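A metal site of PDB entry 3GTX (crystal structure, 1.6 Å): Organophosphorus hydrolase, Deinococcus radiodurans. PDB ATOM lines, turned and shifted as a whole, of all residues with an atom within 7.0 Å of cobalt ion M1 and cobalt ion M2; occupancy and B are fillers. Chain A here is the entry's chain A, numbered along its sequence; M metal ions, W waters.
Within 4 Å of cobalt ion M1: Tyr 113, KCX 159, His 192 and His 220.
Cobalt ion M1 is bound by OQ1 of KCX 159 (2.1 Å), the side-chain hydroxyl of Tyr 113 (2.1 Å), a ring nitrogen (ND1) of His 192 (2.2 Å), a ring nitrogen (NE2) of His 220 (2.3 Å), water W1 (2.3 Å) and water W2 (2.4 Å).
A ring nitrogen (ND1) of His 39 sits at hydrogen-bond distance from the side-chain hydroxyl (OG1) of Thr 84.
The backbone NH (N) of His 39 sits at hydrogen-bond distance from the backbone carbonyl oxygen (O) of Ser 281 (2.9 Å).
The backbone carbonyl oxygen of Ala 83 sits close to NZ of KCX 159, 3.0 Å away.
The guanidinium group (NE) of Arg 244 lies within salt-bridge range of the side-chain carboxylate (OD2) of Asp 280, at 3.0 Å.
N of Asp 280 is in hydrogen-bond range of O of Asp 243 (2.9 Å).
A ring nitrogen (NE2) of His 192 is in hydrogen-bond range of the side-chain amide oxygen (OE1) of Gln 194 (3.1 Å).
O of His 220 lies within hydrogen-bond range of OG1 of Thr 193, at 3.3 Å.
A ring nitrogen (ND1) of His 220 sits at hydrogen-bond distance from the side-chain carboxylate (OD1) of Asp 243, at 2.5 Å.
Cobalt ion M2 is bound by water W1 (1.7 Å), a ring nitrogen (NE2) of His 39 (2.0 Å), OQ2 of KCX 159 (2.1 Å), a ring nitrogen (NE2) of His 37 (2.1 Å) and the side-chain carboxylate of Asp 280 (2.2 Å).
Cobalt ion M2 has five donor atoms within binding distance.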
ATOM      1  N   HIS A  37     -27.988  29.182  17.705  1.00  0.00           N
ATOM      2  CA  HIS A  37     -27.087  28.722  16.691  1.00  0.00           C
ATOM      3  C   HIS A  37     -27.621  27.297  16.266  1.00  0.00           C
ATOM      4  O   HIS A  37     -27.325  26.316  16.905  1.00  0.00           O
ATOM      5  CB  HIS A  37     -25.663  28.571  17.241  1.00  0.00           C
ATOM      6  CG  HIS A  37     -24.685  28.174  16.202  1.00  0.00           C
ATOM      7  ND1 HIS A  37     -23.608  28.967  15.804  1.00  0.00           N
ATOM      8  CD2 HIS A  37     -24.662  27.090  15.386  1.00  0.00           C
ATOM      9  CE1 HIS A  37     -22.987  28.379  14.781  1.00  0.00           C
ATOM     10  NE2 HIS A  37     -23.606  27.226  14.526  1.00  0.00           N
ATOM     11  N   GLU A  38     -28.295  27.334  15.145  1.00  0.00           N
ATOM     12  CA  GLU A  38     -28.887  26.102  14.522  1.00  0.00           C
ATOM     13  C   GLU A  38     -28.804  26.242  13.001  1.00  0.00           C
ATOM     14  O   GLU A  38     -28.465  27.294  12.451  1.00  0.00           O
ATOM     15  CB  GLU A  38     -30.348  26.021  14.958  1.00  0.00           C
ATOM     16  CG  GLU A  38     -30.641  25.887  16.525  1.00  0.00           C
ATOM     17  CD  GLU A  38     -29.948  24.722  17.242  1.00  0.00           C
ATOM     18  OE1 GLU A  38     -29.778  23.659  16.581  1.00  0.00           O
ATOM     19  OE2 GLU A  38     -29.562  24.850  18.459  1.00  0.00           O
ATOM     20  N   HIS A  39     -29.059  25.150  12.269  1.00  0.00           N
ATOM     21  CA  HIS A  39     -29.028  25.204  10.820  1.00  0.00           C
ATOM     22  C   HIS A  39     -30.286  24.548  10.238  1.00  0.00           C
ATOM     23  O   HIS A  39     -30.414  23.319  10.338  1.00  0.00           O
ATOM     24  CB  HIS A  39     -27.793  24.492  10.324  1.00  0.00           C
ATOM     25  CG  HIS A  39     -26.521  25.173  10.766  1.00  0.00           C
ATOM     26  ND1 HIS A  39     -26.057  26.354  10.174  1.00  0.00           N
ATOM     27  CD2 HIS A  39     -25.594  24.813  11.678  1.00  0.00           C
ATOM     28  CE1 HIS A  39     -24.892  26.667  10.719  1.00  0.00           C
ATOM     29  NE2 HIS A  39     -24.582  25.757  11.636  1.00  0.00           N
ATOM     30  N   PHE A  42     -28.288  22.619   5.701  1.00  0.00           N
ATOM     31  CA  PHE A  42     -26.849  22.859   5.650  1.00  0.00           C
ATOM     32  C   PHE A  42     -26.154  21.866   4.729  1.00  0.00           C
ATOM     33  O   PHE A  42     -26.498  20.673   4.693  1.00  0.00           O
ATOM     34  CB  PHE A  42     -26.255  22.732   7.051  1.00  0.00           C
ATOM     35  CG  PHE A  42     -24.772  22.981   7.108  1.00  0.00           C
ATOM     36  CD1 PHE A  42     -23.875  21.943   6.804  1.00  0.00           C
ATOM     37  CD2 PHE A  42     -24.238  24.247   7.502  1.00  0.00           C
ATOM     38  CE1 PHE A  42     -22.481  22.089   6.873  1.00  0.00           C
ATOM     39  CE2 PHE A  42     -22.809  24.417   7.574  1.00  0.00           C
ATOM     40  CZ  PHE A  42     -21.926  23.317   7.258  1.00  0.00           C
ATOM     41  N   ALA A  83     -27.424  30.014  11.708  1.00  0.00           N
ATOM     42  CA  ALA A  83     -26.003  30.422  11.612  1.00  0.00           C
ATOM     43  C   ALA A  83     -25.270  29.996  10.296  1.00  0.00           C
ATOM     44  O   ALA A  83     -24.060  30.118  10.161  1.00  0.00           O
ATOM     45  CB  ALA A  83     -25.297  29.842  12.772  1.00  0.00           C
ATOM     46  N   THR A  84     -26.042  29.526   9.316  1.00  0.00           N
ATOM     47  CA  THR A  84     -25.480  29.040   8.081  1.00  0.00           C
ATOM     48  C   THR A  84     -24.775  30.092   7.247  1.00  0.00           C
ATOM     49  O   THR A  84     -25.413  31.044   6.783  1.00  0.00           O
ATOM     50  CB  THR A  84     -26.565  28.418   7.168  1.00  0.00           C
ATOM     51  OG1 THR A  84     -27.376  27.566   7.992  1.00  0.00           O
ATOM     52  CG2 THR A  84     -25.912  27.600   6.003  1.00  0.00           C
ATOM     53  N   PRO A  85     -23.500  29.870   6.982  1.00  0.00           N
ATOM     54  CA  PRO A  85     -22.691  30.777   6.163  1.00  0.00           C
ATOM     55  C   PRO A  85     -23.141  30.787   4.706  1.00  0.00           C
ATOM     56  O   PRO A  85     -23.814  29.855   4.186  1.00  0.00           O
ATOM     57  CB  PRO A  85     -21.274  30.265   6.298  1.00  0.00           C
ATOM     58  CG  PRO A  85     -21.277  29.400   7.519  1.00  0.00           C
ATOM     59  CD  PRO A  85     -22.678  28.776   7.543  1.00  0.00           C
ATOM     60  N   TYR A 113     -17.499  30.891   6.002  1.00  0.00           N
ATOM     61  CA  TYR A 113     -16.968  30.035   7.060  1.00  0.00           C
ATOM     62  C   TYR A 113     -15.479  30.155   7.208  1.00  0.00           C
ATOM     63  O   TYR A 113     -14.831  30.925   6.493  1.00  0.00           O
ATOM     64  CB  TYR A 113     -17.359  28.547   6.806  1.00  0.00           C
ATOM     65  CG  TYR A 113     -17.717  27.705   8.038  1.00  0.00           C
ATOM     66  CD1 TYR A 113     -18.058  28.293   9.256  1.00  0.00           C
ATOM     67  CD2 TYR A 113     -17.841  26.288   7.934  1.00  0.00           C
ATOM     68  CE1 TYR A 113     -18.523  27.541  10.375  1.00  0.00           C
ATOM     69  CE2 TYR A 113     -18.297  25.543   9.024  1.00  0.00           C
ATOM     70  CZ  TYR A 113     -18.637  26.170  10.228  1.00  0.00           C
ATOM     71  OH  TYR A 113     -19.071  25.517  11.309  1.00  0.00           O
ATOM     72  N   TYR A 114     -14.938  29.420   8.172  1.00  0.00           N
ATOM     73  CA  TYR A 114     -13.517  29.503   8.435  1.00  0.00           C
ATOM     74  C   TYR A 114     -12.716  28.997   7.235  1.00  0.00           C
ATOM     75  O   TYR A 114     -13.199  28.224   6.437  1.00  0.00           O
ATOM     76  CB  TYR A 114     -13.143  28.762   9.743  1.00  0.00           C
ATOM     77  CG  TYR A 114     -13.240  27.258   9.693  1.00  0.00           C
ATOM     78  CD1 TYR A 114     -14.467  26.618   9.765  1.00  0.00           C
ATOM     79  CD2 TYR A 114     -12.098  26.472   9.602  1.00  0.00           C
ATOM     80  CE1 TYR A 114     -14.555  25.214   9.755  1.00  0.00           C
ATOM     81  CE2 TYR A 114     -12.196  25.081   9.575  1.00  0.00           C
ATOM     82  CZ  TYR A 114     -13.416  24.476   9.648  1.00  0.00           C
ATOM     83  OH  TYR A 114     -13.499  23.101   9.571  1.00  0.00           O
ATOM     84  N   KCX A 159     -22.259  36.329  10.667  1.00  0.00           N
ATOM     85  CA  KCX A 159     -21.596  35.119  11.143  1.00  0.00           C
ATOM     86  CB  KCX A 159     -22.253  33.837  10.450  1.00  0.00           C
ATOM     87  CG  KCX A 159     -21.364  32.533  10.628  1.00  0.00           C
ATOM     88  CD  KCX A 159     -21.349  31.947  12.044  1.00  0.00           C
ATOM     89  CE  KCX A 159     -20.665  30.596  12.176  1.00  0.00           C
ATOM     90  NZ  KCX A 159     -21.577  29.522  11.757  1.00  0.00           N
ATOM     91  C   KCX A 159     -20.093  35.171  10.805  1.00  0.00           C
ATOM     92  O   KCX A 159     -19.711  35.287   9.624  1.00  0.00           O
ATOM     93  CX  KCX A 159     -21.431  28.229  12.022  1.00  0.00           C
ATOM     94  OQ1 KCX A 159     -20.551  27.788  12.797  1.00  0.00           O
ATOM     95  OQ2 KCX A 159     -22.294  27.419  11.603  1.00  0.00           O
ATOM     96  N   ALA A 161     -16.072  33.230  11.591  1.00  0.00           N
ATOM     97  CA  ALA A 161     -15.463  31.991  11.977  1.00  0.00           C
ATOM     98  C   ALA A 161     -13.952  32.004  11.824  1.00  0.00           C
ATOM     99  O   ALA A 161     -13.410  32.538  10.858  1.00  0.00           O
ATOM    100  CB  ALA A 161     -16.044  30.866  11.108  1.00  0.00           C
ATOM    101  N   THR A 191     -20.209  33.926  16.393  1.00  0.00           N
ATOM    102  CA  THR A 191     -19.055  33.267  15.866  1.00  0.00           C
ATOM    103  C   THR A 191     -18.975  31.755  15.987  1.00  0.00           C
ATOM    104  O   THR A 191     -19.772  31.137  16.731  1.00  0.00           O
ATOM    105  CB  THR A 191     -17.730  33.811  16.433  1.00  0.00           C
ATOM    106  OG1 THR A 191     -17.361  33.111  17.602  1.00  0.00           O
ATOM    107  CG2 THR A 191     -17.889  35.297  16.720  1.00  0.00           C
ATOM    108  N   HIS A 192     -17.984  31.218  15.252  1.00  0.00           N
ATOM    109  CA  HIS A 192     -17.577  29.832  15.216  1.00  0.00           C
ATOM    110  C   HIS A 192     -16.125  29.816  15.700  1.00  0.00           C
ATOM    111  O   HIS A 192     -15.293  30.569  15.204  1.00  0.00           O
ATOM    112  CB  HIS A 192     -17.545  29.315  13.771  1.00  0.00           C
ATOM    113  CG  HIS A 192     -16.738  28.062  13.598  1.00  0.00           C
ATOM    114  ND1 HIS A 192     -17.328  26.833  13.352  1.00  0.00           N
ATOM    115  CD2 HIS A 192     -15.399  27.851  13.473  1.00  0.00           C
ATOM    116  CE1 HIS A 192     -16.392  25.940  13.054  1.00  0.00           C
ATOM    117  NE2 HIS A 192     -15.212  26.540  13.107  1.00  0.00           N
ATOM    118  N   THR A 193     -15.781  28.916  16.609  1.00  0.00           N
ATOM    119  CA  THR A 193     -14.383  28.725  16.985  1.00  0.00           C
ATOM    120  C   THR A 193     -14.122  27.293  16.597  1.00  0.00           C
ATOM    121  O   THR A 193     -15.037  26.461  16.653  1.00  0.00           O
ATOM    122  CB  THR A 193     -14.100  28.896  18.482  1.00  0.00           C
ATOM    123  OG1 THR A 193     -15.013  28.090  19.278  1.00  0.00           O
ATOM    124  CG2 THR A 193     -14.219  30.383  18.810  1.00  0.00           C
ATOM    125  N   GLN A 194     -12.887  26.991  16.232  1.00  0.00           N
ATOM    126  CA  GLN A 194     -12.535  25.668  15.766  1.00  0.00           C
ATOM    127  C   GLN A 194     -11.772  24.902  16.791  1.00  0.00           C
ATOM    128  O   GLN A 194     -10.749  25.371  17.236  1.00  0.00           O
ATOM    129  CB  GLN A 194     -11.701  25.849  14.501  1.00  0.00           C
ATOM    130  CG  GLN A 194     -11.133  24.603  13.919  1.00  0.00           C
ATOM    131  CD  GLN A 194     -12.229  23.706  13.366  1.00  0.00           C
ATOM    132  OE1 GLN A 194     -13.288  24.177  12.925  1.00  0.00           O
ATOM    133  NE2 GLN A 194     -11.958  22.421  13.357  1.00  0.00           N
ATOM    134  N   HIS A 220     -19.233  27.993  19.832  1.00  0.00           N
ATOM    135  CA  HIS A 220     -18.525  26.737  20.055  1.00  0.00           C
ATOM    136  C   HIS A 220     -17.537  26.723  21.242  1.00  0.00           C
ATOM    137  O   HIS A 220     -16.559  25.994  21.259  1.00  0.00           O
ATOM    138  CB  HIS A 220     -17.814  26.216  18.781  1.00  0.00           C
ATOM    139  CG  HIS A 220     -18.677  26.243  17.563  1.00  0.00           C
ATOM    140  ND1 HIS A 220     -20.051  26.266  17.632  1.00  0.00           N
ATOM    141  CD2 HIS A 220     -18.379  26.272  16.228  1.00  0.00           C
ATOM    142  CE1 HIS A 220     -20.558  26.314  16.410  1.00  0.00           C
ATOM    143  NE2 HIS A 220     -19.565  26.322  15.554  1.00  0.00           N
ATOM    144  N   ASP A 243     -22.856  25.852  22.171  1.00  0.00           N
ATOM    145  CA  ASP A 243     -23.852  25.732  21.113  1.00  0.00           C
ATOM    146  C   ASP A 243     -23.773  24.478  20.228  1.00  0.00           C
ATOM    147  O   ASP A 243     -24.353  24.479  19.142  1.00  0.00           O
ATOM    148  CB  ASP A 243     -23.859  26.989  20.230  1.00  0.00           C
ATOM    149  CG  ASP A 243     -22.450  27.331  19.649  1.00  0.00           C
ATOM    150  OD1 ASP A 243     -21.571  26.435  19.601  1.00  0.00           O
ATOM    151  OD2 ASP A 243     -22.233  28.495  19.242  1.00  0.00           O
ATOM    152  N   ARG A 244     -23.054  23.471  20.668  1.00  0.00           N
ATOM    153  CA  ARG A 244     -22.969  22.176  19.922  1.00  0.00           C
ATOM    154  C   ARG A 244     -23.432  21.076  20.895  1.00  0.00           C
ATOM    155  O   ARG A 244     -22.959  19.943  20.833  1.00  0.00           O
ATOM    156  CB  ARG A 244     -21.537  21.889  19.436  1.00  0.00           C
ATOM    157  CG  ARG A 244     -20.937  23.085  18.674  1.00  0.00           C
ATOM    158  CD  ARG A 244     -19.759  22.710  17.858  1.00  0.00           C
ATOM    159  NE  ARG A 244     -20.143  22.060  16.619  1.00  0.00           N
ATOM    160  CZ  ARG A 244     -19.296  21.307  15.948  1.00  0.00           C
ATOM    161  NH1 ARG A 244     -18.066  21.138  16.420  1.00  0.00           N
ATOM    162  NH2 ARG A 244     -19.669  20.740  14.818  1.00  0.00           N
ATOM    163  N   ASP A 280     -26.339  23.422  17.352  1.00  0.00           N
ATOM    164  CA  ASP A 280     -25.615  23.458  16.082  1.00  0.00           C
ATOM    165  C   ASP A 280     -26.153  22.272  15.259  1.00  0.00           C
ATOM    166  O   ASP A 280     -25.417  21.658  14.513  1.00  0.00           O
ATOM    167  CB  ASP A 280     -24.113  23.322  16.268  1.00  0.00           C
ATOM    168  CG  ASP A 280     -23.339  23.713  15.013  1.00  0.00           C
ATOM    169  OD1 ASP A 280     -23.907  24.409  14.150  1.00  0.00           O
ATOM    170  OD2 ASP A 280     -22.208  23.311  14.829  1.00  0.00           O
ATOM    171  N   SER A 281     -27.455  22.019  15.385  1.00  0.00           N
ATOM    172  CA  SER A 281     -28.015  20.873  14.627  1.00  0.00           C
ATOM    173  C   SER A 281     -28.293  21.221  13.165  1.00  0.00           C
ATOM    174  O   SER A 281     -28.334  22.399  12.770  1.00  0.00           O
ATOM    175  CB  SER A 281     -29.306  20.427  15.283  1.00  0.00           C
ATOM    176  OG  SER A 281     -30.304  21.457  15.199  1.00  0.00           O
ATOM    177  N   ILE A 282     -28.536  20.187  12.344  1.00  0.00           N
ATOM    178  CA  ILE A 282     -28.808  20.410  10.940  1.00  0.00           C
ATOM    179  C   ILE A 282     -30.141  19.695  10.759  1.00  0.00           C
ATOM    180  O   ILE A 282     -30.194  18.509  11.023  1.00  0.00           O
ATOM    181  CB  ILE A 282     -27.719  19.809  10.069  1.00  0.00           C
ATOM    182  CG1 ILE A 282     -26.447  20.677  10.208  1.00  0.00           C
ATOM    183  CG2 ILE A 282     -28.167  19.772   8.683  1.00  0.00           C
ATOM    184  CD1 ILE A 282     -25.230  20.053   9.608  1.00  0.00           C
HETATM  185 CO    CO M   1     -19.436  26.121  13.310  1.00  0.00          CO
HETATM  186 CO    CO M   2     -23.044  25.983  12.880  1.00  0.00          CO
HETATM  187  O   HOH W   1     -21.528  25.238  13.213  1.00  0.00           O
HETATM  188  O   HOH W   2     -18.587  23.961  13.852  1.00  0.00           O
